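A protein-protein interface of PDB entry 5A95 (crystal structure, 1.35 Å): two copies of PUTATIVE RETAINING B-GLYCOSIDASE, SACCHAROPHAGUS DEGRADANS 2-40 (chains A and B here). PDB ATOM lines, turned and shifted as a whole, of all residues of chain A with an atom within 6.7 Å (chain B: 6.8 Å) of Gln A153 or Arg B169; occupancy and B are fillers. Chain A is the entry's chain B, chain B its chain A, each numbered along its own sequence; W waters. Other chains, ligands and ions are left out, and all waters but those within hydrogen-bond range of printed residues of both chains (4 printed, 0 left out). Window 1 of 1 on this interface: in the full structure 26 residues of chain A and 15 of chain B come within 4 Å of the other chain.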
ATOM      1  N   SER A 143       9.444  -0.277  -1.463  1.00  0.00           N
ATOM      2  CA  SER A 143       9.451   1.071  -0.915  1.00  0.00           C
ATOM      3  C   SER A 143       9.482   2.083  -2.052  1.00  0.00           C
ATOM      4  O   SER A 143       9.760   1.738  -3.199  1.00  0.00           O
ATOM      5  CB  SER A 143      10.655   1.221   0.028  1.00  0.00           C
ATOM      6  OG  SER A 143      10.679   2.498   0.659  1.00  0.00           O
ATOM      7  N   ILE A 144       9.128   3.309  -1.718  1.00  0.00           N
ATOM      8  CA  ILE A 144       9.071   4.412  -2.656  1.00  0.00           C
ATOM      9  C   ILE A 144       9.682   5.597  -1.923  1.00  0.00           C
ATOM     10  O   ILE A 144       9.135   6.053  -0.918  1.00  0.00           O
ATOM     11  CB  ILE A 144       7.627   4.769  -3.102  1.00  0.00           C
ATOM     12  CG1 ILE A 144       6.887   3.555  -3.646  1.00  0.00           C
ATOM     13  CG2 ILE A 144       7.667   5.925  -4.089  1.00  0.00           C
ATOM     14  CD1 ILE A 144       5.507   3.888  -4.149  1.00  0.00           C
ATOM     15  N   GLY A 145      10.813   6.097  -2.410  1.00  0.00           N
ATOM     16  CA  GLY A 145      11.479   7.181  -1.746  1.00  0.00           C
ATOM     17  C   GLY A 145      12.960   7.130  -1.911  1.00  0.00           C
ATOM     18  O   GLY A 145      13.452   6.562  -2.875  1.00  0.00           O
ATOM     19  N   TYR A 146      13.678   7.745  -0.966  1.00  0.00           N
ATOM     20  CA  TYR A 146      15.110   7.949  -1.098  1.00  0.00           C
ATOM     21  C   TYR A 146      15.794   7.297   0.104  1.00  0.00           C
ATOM     22  O   TYR A 146      15.866   7.859   1.197  1.00  0.00           O
ATOM     23  CB  TYR A 146      15.475   9.444  -1.245  1.00  0.00           C
ATOM     24  CG  TYR A 146      16.860   9.643  -1.813  1.00  0.00           C
ATOM     25  CD1 TYR A 146      17.189   9.130  -3.041  1.00  0.00           C
ATOM     26  CD2 TYR A 146      17.843  10.313  -1.104  1.00  0.00           C
ATOM     27  CE1 TYR A 146      18.454   9.284  -3.563  1.00  0.00           C
ATOM     28  CE2 TYR A 146      19.116  10.461  -1.603  1.00  0.00           C
ATOM     29  CZ  TYR A 146      19.422   9.940  -2.855  1.00  0.00           C
ATOM     30  OH  TYR A 146      20.677  10.056  -3.405  1.00  0.00           O
ATOM     31  N   GLN A 151      13.815   8.758   3.726  1.00  0.00           N
ATOM     32  CA  GLN A 151      12.568   9.524   3.584  1.00  0.00           C
ATOM     33  C   GLN A 151      11.762   8.949   2.423  1.00  0.00           C
ATOM     34  O   GLN A 151      12.345   8.616   1.399  1.00  0.00           O
ATOM     35  CB  GLN A 151      12.862  11.003   3.313  1.00  0.00           C
ATOM     36  CG  GLN A 151      13.804  11.663   4.317  1.00  0.00           C
ATOM     37  CD  GLN A 151      13.254  11.755   5.718  1.00  0.00           C
ATOM     38  OE1 GLN A 151      12.246  12.388   5.932  1.00  0.00           O
ATOM     39  NE2 GLN A 151      13.948  11.123   6.693  1.00  0.00           N
ATOM     40  N   TYR A 152      10.437   8.902   2.588  1.00  0.00           N
ATOM     41  CA  TYR A 152       9.584   8.116   1.700  1.00  0.00           C
ATOM     42  C   TYR A 152       8.304   8.809   1.289  1.00  0.00           C
ATOM     43  O   TYR A 152       7.878   9.781   1.894  1.00  0.00           O
ATOM     44  CB  TYR A 152       9.265   6.749   2.363  1.00  0.00           C
ATOM     45  CG  TYR A 152      10.537   6.064   2.794  1.00  0.00           C
ATOM     46  CD1 TYR A 152      11.323   5.344   1.890  1.00  0.00           C
ATOM     47  CD2 TYR A 152      10.986   6.190   4.103  1.00  0.00           C
ATOM     48  CE1 TYR A 152      12.525   4.797   2.288  1.00  0.00           C
ATOM     49  CE2 TYR A 152      12.192   5.651   4.489  1.00  0.00           C
ATOM     50  CZ  TYR A 152      12.950   4.944   3.600  1.00  0.00           C
ATOM     51  OH  TYR A 152      14.170   4.424   3.986  1.00  0.00           O
ATOM     52  N   GLN A 153       7.664   8.240   0.288  1.00  0.00           N
ATOM     53  CA  GLN A 153       6.416   8.805  -0.203  1.00  0.00           C
ATOM     54  C   GLN A 153       5.247   8.706   0.789  1.00  0.00           C
ATOM     55  O   GLN A 153       4.368   9.561   0.831  1.00  0.00           O
ATOM     56  CB  GLN A 153       6.066   8.148  -1.541  1.00  0.00           C
ATOM     57  CG  GLN A 153       4.731   8.588  -2.096  1.00  0.00           C
ATOM     58  CD  GLN A 153       4.544   8.161  -3.534  1.00  0.00           C
ATOM     59  OE1 GLN A 153       5.340   8.536  -4.398  1.00  0.00           O
ATOM     60  NE2 GLN A 153       3.506   7.378  -3.781  1.00  0.00           N
ATOM     61  N   HIS A 154       5.229   7.620   1.561  1.00  0.00           N
ATOM     62  CA  HIS A 154       4.114   7.325   2.464  1.00  0.00           C
ATOM     63  C   HIS A 154       4.661   6.370   3.535  1.00  0.00           C
ATOM     64  O   HIS A 154       5.560   5.565   3.266  1.00  0.00           O
ATOM     65  CB  HIS A 154       2.990   6.651   1.666  1.00  0.00           C
ATOM     66  CG  HIS A 154       1.745   6.369   2.450  1.00  0.00           C
ATOM     67  ND1 HIS A 154       1.653   5.343   3.368  1.00  0.00           N
ATOM     68  CD2 HIS A 154       0.512   6.934   2.388  1.00  0.00           C
ATOM     69  CE1 HIS A 154       0.437   5.323   3.875  1.00  0.00           C
ATOM     70  NE2 HIS A 154      -0.275   6.283   3.301  1.00  0.00           N
ATOM     71  N   PRO A 155       4.112   6.415   4.758  1.00  0.00           N
ATOM     72  CA  PRO A 155       4.563   5.499   5.818  1.00  0.00           C
ATOM     73  C   PRO A 155       4.487   4.011   5.518  1.00  0.00           C
ATOM     74  O   PRO A 155       5.267   3.269   6.095  1.00  0.00           O
ATOM     75  CB  PRO A 155       3.701   5.898   7.017  1.00  0.00           C
ATOM     76  CG  PRO A 155       3.389   7.344   6.791  1.00  0.00           C
ATOM     77  CD  PRO A 155       3.239   7.474   5.294  1.00  0.00           C
ATOM     78  N   MET A 156       3.644   3.552   4.599  1.00  0.00           N
ATOM     79  CA  MET A 156       3.604   2.135   4.318  1.00  0.00           C
ATOM     80  C   MET A 156       4.926   1.671   3.729  1.00  0.00           C
ATOM     81  O   MET A 156       5.227   0.472   3.756  1.00  0.00           O
ATOM     82  CB  MET A 156       2.443   1.733   3.401  1.00  0.00           C
ATOM     83  CG  MET A 156       2.490   2.311   2.003  1.00  0.00           C
ATOM     84  SD  MET A 156       1.117   1.764   0.955  1.00  0.00           S
ATOM     85  CE  MET A 156      -0.230   2.776   1.591  1.00  0.00           C
ATOM     86  N   TYR A 157       5.688   2.621   3.163  1.00  0.00           N
ATOM     87  CA  TYR A 157       6.956   2.318   2.528  1.00  0.00           C
ATOM     88  C   TYR A 157       8.155   2.595   3.453  1.00  0.00           C
ATOM     89  O   TYR A 157       9.306   2.424   3.065  1.00  0.00           O
ATOM     90  CB  TYR A 157       7.110   3.165   1.268  1.00  0.00           C
ATOM     91  CG  TYR A 157       5.923   3.064   0.318  1.00  0.00           C
ATOM     92  CD1 TYR A 157       5.525   1.833  -0.186  1.00  0.00           C
ATOM     93  CD2 TYR A 157       5.206   4.193  -0.069  1.00  0.00           C
ATOM     94  CE1 TYR A 157       4.426   1.710  -1.023  1.00  0.00           C
ATOM     95  CE2 TYR A 157       4.106   4.092  -0.902  1.00  0.00           C
ATOM     96  CZ  TYR A 157       3.726   2.854  -1.379  1.00  0.00           C
ATOM     97  OH  TYR A 157       2.633   2.756  -2.194  1.00  0.00           O
ATOM     98  N   GLU A 189      11.033   1.784  -5.983  1.00  0.00           N
ATOM     99  CA  GLU A 189      10.958   3.050  -6.700  1.00  0.00           C
ATOM    100  C   GLU A 189      11.763   4.152  -6.008  1.00  0.00           C
ATOM    101  O   GLU A 189      11.255   4.884  -5.156  1.00  0.00           O
ATOM    102  CB  GLU A 189       9.504   3.484  -6.895  1.00  0.00           C
ATOM    103  CG  GLU A 189       8.868   2.772  -8.064  1.00  0.00           C
ATOM    104  CD  GLU A 189       7.446   3.169  -8.363  1.00  0.00           C
ATOM    105  OE1 GLU A 189       6.777   3.747  -7.497  1.00  0.00           O
ATOM    106  OE2 GLU A 189       7.023   2.879  -9.501  1.00  0.00           O
ATOM    107  N   THR A 191      13.033   7.726  -5.623  1.00  0.00           N
ATOM    108  CA  THR A 191      12.545   9.057  -5.951  1.00  0.00           C
ATOM    109  C   THR A 191      12.854   9.982  -4.796  1.00  0.00           C
ATOM    110  O   THR A 191      12.804   9.556  -3.630  1.00  0.00           O
ATOM    111  CB  THR A 191      11.025   9.079  -6.242  1.00  0.00           C
ATOM    112  OG1 THR A 191      10.672  10.436  -6.520  1.00  0.00           O
ATOM    113  CG2 THR A 191      10.174   8.557  -5.108  1.00  0.00           C
ATOM    114  N   MET A 193      11.029  12.923  -4.943  1.00  0.00           N
ATOM    115  CA  MET A 193       9.813  13.743  -5.018  1.00  0.00           C
ATOM    116  C   MET A 193      10.173  15.212  -5.175  1.00  0.00           C
ATOM    117  O   MET A 193       9.785  16.054  -4.379  1.00  0.00           O
ATOM    118  CB  MET A 193       8.913  13.485  -3.817  1.00  0.00           C
ATOM    119  CG  MET A 193       8.550  12.018  -3.641  1.00  0.00           C
ATOM    120  SD  MET A 193       7.407  11.727  -2.242  1.00  0.00           S
ATOM    121  CE  MET A 193       5.855  12.151  -3.014  1.00  0.00           C
ATOM    122  N   THR A 196      12.251  16.963  -2.388  1.00  0.00           N
ATOM    123  CA  THR A 196      11.660  17.151  -1.069  1.00  0.00           C
ATOM    124  C   THR A 196      12.073  16.068  -0.050  1.00  0.00           C
ATOM    125  O   THR A 196      11.933  16.261   1.165  1.00  0.00           O
ATOM    126  CB  THR A 196      10.125  17.216  -1.119  1.00  0.00           C
ATOM    127  OG1 THR A 196       9.605  15.982  -1.641  1.00  0.00           O
ATOM    128  CG2 THR A 196       9.655  18.384  -1.957  1.00  0.00           C
ATOM    129  N   LEU A 197      12.546  14.916  -0.534  1.00  0.00           N
ATOM    130  CA  LEU A 197      12.963  13.820   0.338  1.00  0.00           C
ATOM    131  C   LEU A 197      14.452  13.801   0.615  1.00  0.00           C
ATOM    132  O   LEU A 197      14.897  13.013   1.458  1.00  0.00           O
ATOM    133  CB  LEU A 197      12.545  12.487  -0.269  1.00  0.00           C
ATOM    134  CG  LEU A 197      11.048  12.282  -0.500  1.00  0.00           C
ATOM    135  CD1 LEU A 197      10.785  10.853  -0.920  1.00  0.00           C
ATOM    136  CD2 LEU A 197      10.205  12.627   0.696  1.00  0.00           C
ATOM    137  N   TRP A 232      11.047   7.551  -9.810  1.00  0.00           N
ATOM    138  CA  TRP A 232      10.227   6.364  -9.566  1.00  0.00           C
ATOM    139  C   TRP A 232      10.589   5.227 -10.511  1.00  0.00           C
ATOM    140  O   TRP A 232       9.752   4.631 -11.153  1.00  0.00           O
ATOM    141  CB  TRP A 232       8.724   6.673  -9.639  1.00  0.00           C
ATOM    142  CG  TRP A 232       8.125   7.533  -8.538  1.00  0.00           C
ATOM    143  CD1 TRP A 232       7.380   7.089  -7.485  1.00  0.00           C
ATOM    144  CD2 TRP A 232       8.093   8.981  -8.441  1.00  0.00           C
ATOM    145  NE1 TRP A 232       6.918   8.149  -6.725  1.00  0.00           N
ATOM    146  CE2 TRP A 232       7.322   9.318  -7.299  1.00  0.00           C
ATOM    147  CE3 TRP A 232       8.618  10.007  -9.216  1.00  0.00           C
ATOM    148  CZ2 TRP A 232       7.100  10.631  -6.910  1.00  0.00           C
ATOM    149  CZ3 TRP A 232       8.400  11.321  -8.822  1.00  0.00           C
ATOM    150  CH2 TRP A 232       7.644  11.619  -7.687  1.00  0.00           C
ATOM    151  N   TYR B  36      -2.942   9.632   2.482  1.00  0.00           N
ATOM    152  CA  TYR B  36      -1.878  10.584   2.267  1.00  0.00           C
ATOM    153  C   TYR B  36      -2.165  11.842   3.076  1.00  0.00           C
ATOM    154  O   TYR B  36      -3.330  12.154   3.326  1.00  0.00           O
ATOM    155  CB  TYR B  36      -1.728  10.883   0.777  1.00  0.00           C
ATOM    156  CG  TYR B  36      -0.891   9.831   0.089  1.00  0.00           C
ATOM    157  CD1 TYR B  36      -1.440   8.626  -0.298  1.00  0.00           C
ATOM    158  CD2 TYR B  36       0.437  10.039  -0.129  1.00  0.00           C
ATOM    159  CE1 TYR B  36      -0.667   7.627  -0.867  1.00  0.00           C
ATOM    160  CE2 TYR B  36       1.221   9.068  -0.719  1.00  0.00           C
ATOM    161  CZ  TYR B  36       0.681   7.854  -1.087  1.00  0.00           C
ATOM    162  OH  TYR B  36       1.490   6.892  -1.654  1.00  0.00           O
ATOM    163  N   PRO B  37      -1.121  12.575   3.466  1.00  0.00           N
ATOM    164  CA  PRO B  37      -1.342  13.771   4.268  1.00  0.00           C
ATOM    165  C   PRO B  37      -1.953  14.931   3.481  1.00  0.00           C
ATOM    166  O   PRO B  37      -1.833  14.976   2.253  1.00  0.00           O
ATOM    167  CB  PRO B  37       0.067  14.138   4.732  1.00  0.00           C
ATOM    168  CG  PRO B  37       0.968  13.627   3.659  1.00  0.00           C
ATOM    169  CD  PRO B  37       0.309  12.331   3.223  1.00  0.00           C
ATOM    170  N   THR B 164      14.379  13.907  12.379  1.00  0.00           N
ATOM    171  CA  THR B 164      14.497  15.356  12.157  1.00  0.00           C
ATOM    172  C   THR B 164      14.106  15.765  10.753  1.00  0.00           C
ATOM    173  O   THR B 164      13.306  16.681  10.545  1.00  0.00           O
ATOM    174  CB  THR B 164      15.937  15.816  12.496  1.00  0.00           C
ATOM    175  OG1 THR B 164      16.194  15.549  13.899  1.00  0.00           O
ATOM    176  CG2 THR B 164      16.139  17.286  12.213  1.00  0.00           C
ATOM    177  N   ARG B 165      14.649  15.054   9.781  1.00  0.00           N
ATOM    178  CA  ARG B 165      14.276  15.274   8.377  1.00  0.00           C
ATOM    179  C   ARG B 165      12.767  15.093   8.198  1.00  0.00           C
ATOM    180  O   ARG B 165      12.123  15.878   7.504  1.00  0.00           O
ATOM    181  CB  ARG B 165      14.988  14.275   7.466  1.00  0.00           C
ATOM    182  CG  ARG B 165      16.460  14.502   7.243  1.00  0.00           C
ATOM    183  CD  ARG B 165      16.945  13.513   6.194  1.00  0.00           C
ATOM    184  NE  ARG B 165      18.377  13.503   6.045  1.00  0.00           N
ATOM    185  CZ  ARG B 165      19.079  14.420   5.408  1.00  0.00           C
ATOM    186  NH1 ARG B 165      18.464  15.402   4.745  1.00  0.00           N
ATOM    187  NH2 ARG B 165      20.400  14.331   5.373  1.00  0.00           N
ATOM    188  N   ASP B 166      12.214  14.032   8.779  1.00  0.00           N
ATOM    189  CA  ASP B 166      10.795  13.757   8.614  1.00  0.00           C
ATOM    190  C   ASP B 166       9.912  14.825   9.241  1.00  0.00           C
ATOM    191  O   ASP B 166       8.884  15.200   8.673  1.00  0.00           O
ATOM    192  CB  ASP B 166      10.442  12.362   9.122  1.00  0.00           C
ATOM    193  CG  ASP B 166       8.963  12.103   9.097  1.00  0.00           C
ATOM    194  OD1 ASP B 166       8.433  11.868   7.987  1.00  0.00           O
ATOM    195  OD2 ASP B 166       8.307  12.156  10.150  1.00  0.00           O
ATOM    196  N   PHE B 167      10.306  15.305  10.415  1.00  0.00           N
ATOM    197  CA  PHE B 167       9.633  16.435  11.020  1.00  0.00           C
ATOM    198  C   PHE B 167       9.562  17.612  10.056  1.00  0.00           C
ATOM    199  O   PHE B 167       8.481  18.145   9.777  1.00  0.00           O
ATOM    200  CB  PHE B 167      10.279  16.817  12.357  1.00  0.00           C
ATOM    201  CG  PHE B 167       9.758  18.088  12.962  1.00  0.00           C
ATOM    202  CD1 PHE B 167       8.570  18.102  13.656  1.00  0.00           C
ATOM    203  CD2 PHE B 167      10.455  19.289  12.807  1.00  0.00           C
ATOM    204  CE1 PHE B 167       8.088  19.276  14.184  1.00  0.00           C
ATOM    205  CE2 PHE B 167       9.974  20.467  13.346  1.00  0.00           C
ATOM    206  CZ  PHE B 167       8.791  20.455  14.038  1.00  0.00           C
ATOM    207  N   TRP B 168      10.715  17.989   9.515  1.00  0.00           N
ATOM    208  CA  TRP B 168      10.734  19.146   8.638  1.00  0.00           C
ATOM    209  C   TRP B 168       9.990  18.873   7.317  1.00  0.00           C
ATOM    210  O   TRP B 168       9.333  19.781   6.780  1.00  0.00           O
ATOM    211  CB  TRP B 168      12.160  19.666   8.425  1.00  0.00           C
ATOM    212  CG  TRP B 168      12.675  20.351   9.651  1.00  0.00           C
ATOM    213  CD1 TRP B 168      13.740  19.974  10.424  1.00  0.00           C
ATOM    214  CD2 TRP B 168      12.086  21.487  10.309  1.00  0.00           C
ATOM    215  NE1 TRP B 168      13.861  20.820  11.485  1.00  0.00           N
ATOM    216  CE2 TRP B 168      12.863  21.763  11.447  1.00  0.00           C
ATOM    217  CE3 TRP B 168      10.963  22.295  10.034  1.00  0.00           C
ATOM    218  CZ2 TRP B 168      12.563  22.793  12.310  1.00  0.00           C
ATOM    219  CZ3 TRP B 168      10.670  23.303  10.906  1.00  0.00           C
ATOM    220  CH2 TRP B 168      11.465  23.550  12.018  1.00  0.00           C
ATOM    221  N   ARG B 169      10.065  17.659   6.780  1.00  0.00           N
ATOM    222  CA  ARG B 169       9.291  17.306   5.594  1.00  0.00           C
ATOM    223  C   ARG B 169       7.798  17.495   5.852  1.00  0.00           C
ATOM    224  O   ARG B 169       7.076  18.131   5.044  1.00  0.00           O
ATOM    225  CB  ARG B 169       9.620  15.859   5.179  1.00  0.00           C
ATOM    226  CG  ARG B 169       8.875  15.346   3.951  1.00  0.00           C
ATOM    227  CD  ARG B 169       7.478  14.773   4.291  1.00  0.00           C
ATOM    228  NE  ARG B 169       6.847  14.195   3.121  1.00  0.00           N
ATOM    229  CZ  ARG B 169       7.086  12.969   2.671  1.00  0.00           C
ATOM    230  NH1 ARG B 169       7.925  12.180   3.299  1.00  0.00           N
ATOM    231  NH2 ARG B 169       6.466  12.523   1.583  1.00  0.00           N
ATOM    232  N   ARG B 170       7.320  16.978   6.970  1.00  0.00           N
ATOM    233  CA  ARG B 170       5.900  17.037   7.281  1.00  0.00           C
ATOM    234  C   ARG B 170       5.431  18.472   7.508  1.00  0.00           C
ATOM    235  O   ARG B 170       4.350  18.871   7.059  1.00  0.00           O
ATOM    236  CB  ARG B 170       5.575  16.222   8.523  1.00  0.00           C
ATOM    237  CG  ARG B 170       5.630  14.719   8.352  1.00  0.00           C
ATOM    238  CD  ARG B 170       5.488  14.079   9.719  1.00  0.00           C
ATOM    239  NE  ARG B 170       5.599  12.629   9.799  1.00  0.00           N
ATOM    240  CZ  ARG B 170       4.571  11.790   9.707  1.00  0.00           C
ATOM    241  NH1 ARG B 170       3.356  12.204   9.447  1.00  0.00           N
ATOM    242  NH2 ARG B 170       4.781  10.508   9.875  1.00  0.00           N
ATOM    243  N   ILE B 171       6.204  19.228   8.265  1.00  0.00           N
ATOM    244  CA  ILE B 171       5.899  20.604   8.569  1.00  0.00           C
ATOM    245  C   ILE B 171       5.842  21.435   7.298  1.00  0.00           C
ATOM    246  O   ILE B 171       4.913  22.236   7.097  1.00  0.00           O
ATOM    247  CB  ILE B 171       6.941  21.179   9.573  1.00  0.00           C
ATOM    248  CG1 ILE B 171       6.818  20.561  10.971  1.00  0.00           C
ATOM    249  CG2 ILE B 171       6.900  22.693   9.606  1.00  0.00           C
ATOM    250  CD1 ILE B 171       5.605  21.032  11.767  1.00  0.00           C
ATOM    251  N   THR B 172       6.856  21.292   6.461  1.00  0.00           N
ATOM    252  CA  THR B 172       6.949  22.130   5.297  1.00  0.00           C
ATOM    253  C   THR B 172       5.812  21.874   4.335  1.00  0.00           C
ATOM    254  O   THR B 172       5.251  22.799   3.750  1.00  0.00           O
ATOM    255  CB  THR B 172       8.323  21.996   4.605  1.00  0.00           C
ATOM    256  OG1 THR B 172       9.378  22.226   5.553  1.00  0.00           O
ATOM    257  CG2 THR B 172       8.477  23.007   3.509  1.00  0.00           C
ATOM    258  N   PHE B 173       5.450  20.605   4.175  1.00  0.00           N
ATOM    259  CA  PHE B 173       4.295  20.264   3.351  1.00  0.00           C
ATOM    260  C   PHE B 173       3.004  20.839   3.933  1.00  0.00           C
ATOM    261  O   PHE B 173       2.217  21.477   3.246  1.00  0.00           O
ATOM    262  CB  PHE B 173       4.160  18.752   3.229  1.00  0.00           C
ATOM    263  CG  PHE B 173       2.938  18.286   2.473  1.00  0.00           C
ATOM    264  CD1 PHE B 173       2.866  18.371   1.102  1.00  0.00           C
ATOM    265  CD2 PHE B 173       1.880  17.733   3.150  1.00  0.00           C
ATOM    266  CE1 PHE B 173       1.752  17.909   0.433  1.00  0.00           C
ATOM    267  CE2 PHE B 173       0.754  17.290   2.491  1.00  0.00           C
ATOM    268  CZ  PHE B 173       0.705  17.379   1.128  1.00  0.00           C
ATOM    269  N   ARG B 174       2.776  20.629   5.213  1.00  0.00           N
ATOM    270  CA  ARG B 174       1.525  21.029   5.804  1.00  0.00           C
ATOM    271  C   ARG B 174       1.306  22.522   5.757  1.00  0.00           C
ATOM    272  O   ARG B 174       0.174  22.967   5.560  1.00  0.00           O
ATOM    273  CB  ARG B 174       1.396  20.551   7.246  1.00  0.00           C
ATOM    274  CG  ARG B 174      -0.016  20.641   7.812  1.00  0.00           C
ATOM    275  CD  ARG B 174      -0.075  19.990   9.175  1.00  0.00           C
ATOM    276  NE  ARG B 174      -1.387  19.866   9.777  1.00  0.00           N
ATOM    277  CZ  ARG B 174      -2.036  18.715   9.968  1.00  0.00           C
ATOM    278  NH1 ARG B 174      -1.582  17.577   9.450  1.00  0.00           N
ATOM    279  NH2 ARG B 174      -3.147  18.692  10.662  1.00  0.00           N
ATOM    280  N   MET B 215      15.825  20.204   1.516  1.00  0.00           N
ATOM    281  CA  MET B 215      14.540  19.518   1.589  1.00  0.00           C
ATOM    282  C   MET B 215      13.390  20.480   1.798  1.00  0.00           C
ATOM    283  O   MET B 215      12.328  20.339   1.214  1.00  0.00           O
ATOM    284  CB  MET B 215      14.466  18.541   2.782  1.00  0.00           C
ATOM    285  CG  MET B 215      15.244  17.276   2.700  1.00  0.00           C
ATOM    286  SD  MET B 215      15.100  16.418   4.288  1.00  0.00           S
ATOM    287  CE  MET B 215      13.394  15.843   4.171  1.00  0.00           C
ATOM    288  N   ILE B 216      13.604  21.444   2.691  1.00  0.00           N
ATOM    289  CA  ILE B 216      12.591  22.433   3.015  1.00  0.00           C
ATOM    290  C   ILE B 216      12.289  23.314   1.792  1.00  0.00           C
ATOM    291  O   ILE B 216      11.126  23.491   1.391  1.00  0.00           O
ATOM    292  CB  ILE B 216      13.030  23.263   4.221  1.00  0.00           C
ATOM    293  CG1 ILE B 216      13.004  22.392   5.489  1.00  0.00           C
ATOM    294  CG2 ILE B 216      12.152  24.491   4.407  1.00  0.00           C
ATOM    295  CD1 ILE B 216      13.726  23.007   6.667  1.00  0.00           C
ATOM    296  N   SER B 219      10.178  22.131  -1.005  1.00  0.00           N
ATOM    297  CA  SER B 219       8.759  22.055  -0.660  1.00  0.00           C
ATOM    298  C   SER B 219       8.109  23.434  -0.468  1.00  0.00           C
ATOM    299  O   SER B 219       6.945  23.593  -0.831  1.00  0.00           O
ATOM    300  CB  SER B 219       8.654  21.190   0.595  1.00  0.00           C
ATOM    301  OG  SER B 219       7.324  21.077   1.051  1.00  0.00           O
HETATM  302  O   HOH W   1       7.219  14.957  -0.705  1.00  0.00           O
HETATM  303  O   HOH W   2       9.544  12.236   5.617  1.00  0.00           O
HETATM  304  O   HOH W   3       4.500  10.558   3.644  1.00  0.00           O
HETATM  305  O   HOH W   4       0.489   4.470  -1.797  1.00  0.00           O
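Ser A143 touches none of the printed residues of chain B.
Of the printed residues of chain B, Tyr A152 touches Arg B169.
Gln A153 touches two residues of chain B.
Of the printed residues of chain B, Thr A196 touches Met B215 and Ser B219.
Printed residues of chain A within 4 Å of Arg B165: Gln A151.
Of the printed residues of chain A, Arg B169 touches Tyr A152, Gln A153 and Leu A197.
Ile B171 touches none of the printed residues of chain A.
No position is printed for both chains.
O of Ile A144 is in hydrogen-bond range of N of Gln A153 (2.9 Å).
The indole nitrogen of Trp A232 sits at hydrogen-bond distance from the side-chain amide oxygen of Gln A153 (2.8 Å).
The guanidinium group (NH1) of Arg B165 sits at hydrogen-bond distance from the side-chain sulfur (SD) of Met B215, 3.5 Å away.
The side-chain hydroxyl (OG) of Ser A143 is in hydrogen-bond range of the backbone carbonyl oxygen (O) of Tyr A157 (2.8 Å).
ND1 of His A154 lies within hydrogen-bond range of N of Met A156 (2.9 Å).
OD2 of Asp B166 is in salt-bridge range of NE of Arg B170 (2.8 Å).
The side-chain hydroxyl (OH) of Tyr B36 is in hydrogen-bond range of the side-chain amide nitrogen (NE2) of Gln A153 (3.0 Å).
The side-chain amide oxygen (OE1) of Gln A151 is in hydrogen-bond range of the backbone NH (N) of Asp B166, 3.3 Å away.
The guanidinium group (NH1) of Arg B169 lies within hydrogen-bond range of the backbone carbonyl oxygen (O) of Tyr A152 (2.8 Å).
Of the 16 printed residues of chain B, 6 touch a printed residue of chain A.
Hydrophobic or aromatic side chains of chain B that line the printed part of chain A: Tyr B36 and Met B215.
Among the printed residues, 10 pairs touch across the chains.
Among the printed residues, no Asp or Glu carboxylate lies within 4 Å of a Lys or Arg side-chain nitrogen of the other chain.
Gln A151 touches Arg B165.
Gln A153 touches Arg B169.
His A154 touches Tyr B36 (CD2 to CE1, 3.5 Å).
CE2 of Tyr A157 touches OH of Tyr B36, at 3.9 Å.
Thr A196 touches Met B215.
Thr A196 touches Ser B219 (CG2 to N, 3.9 Å).
Arg B169 touches Leu A197.
Water W4 lies within hydrogen-bond range of OH of Tyr B36 and OH of Tyr A157.
Water W2 lies within hydrogen-bond range of OD1 of Asp B166 (2.6 Å), OE1 of Gln A151 (2.7 Å) and NH1 of Arg B169 (2.8 Å).
Water W1 lies within hydrogen-bond range of the side-chain hydroxyl (OG1) of Thr A196, the guanidinium group (NH2) of Arg B169 and the side-chain sulfur (SD) of Met A193.
Water W3 lies within hydrogen-bond range of O of Gln A153 and NH2 of Arg B169.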
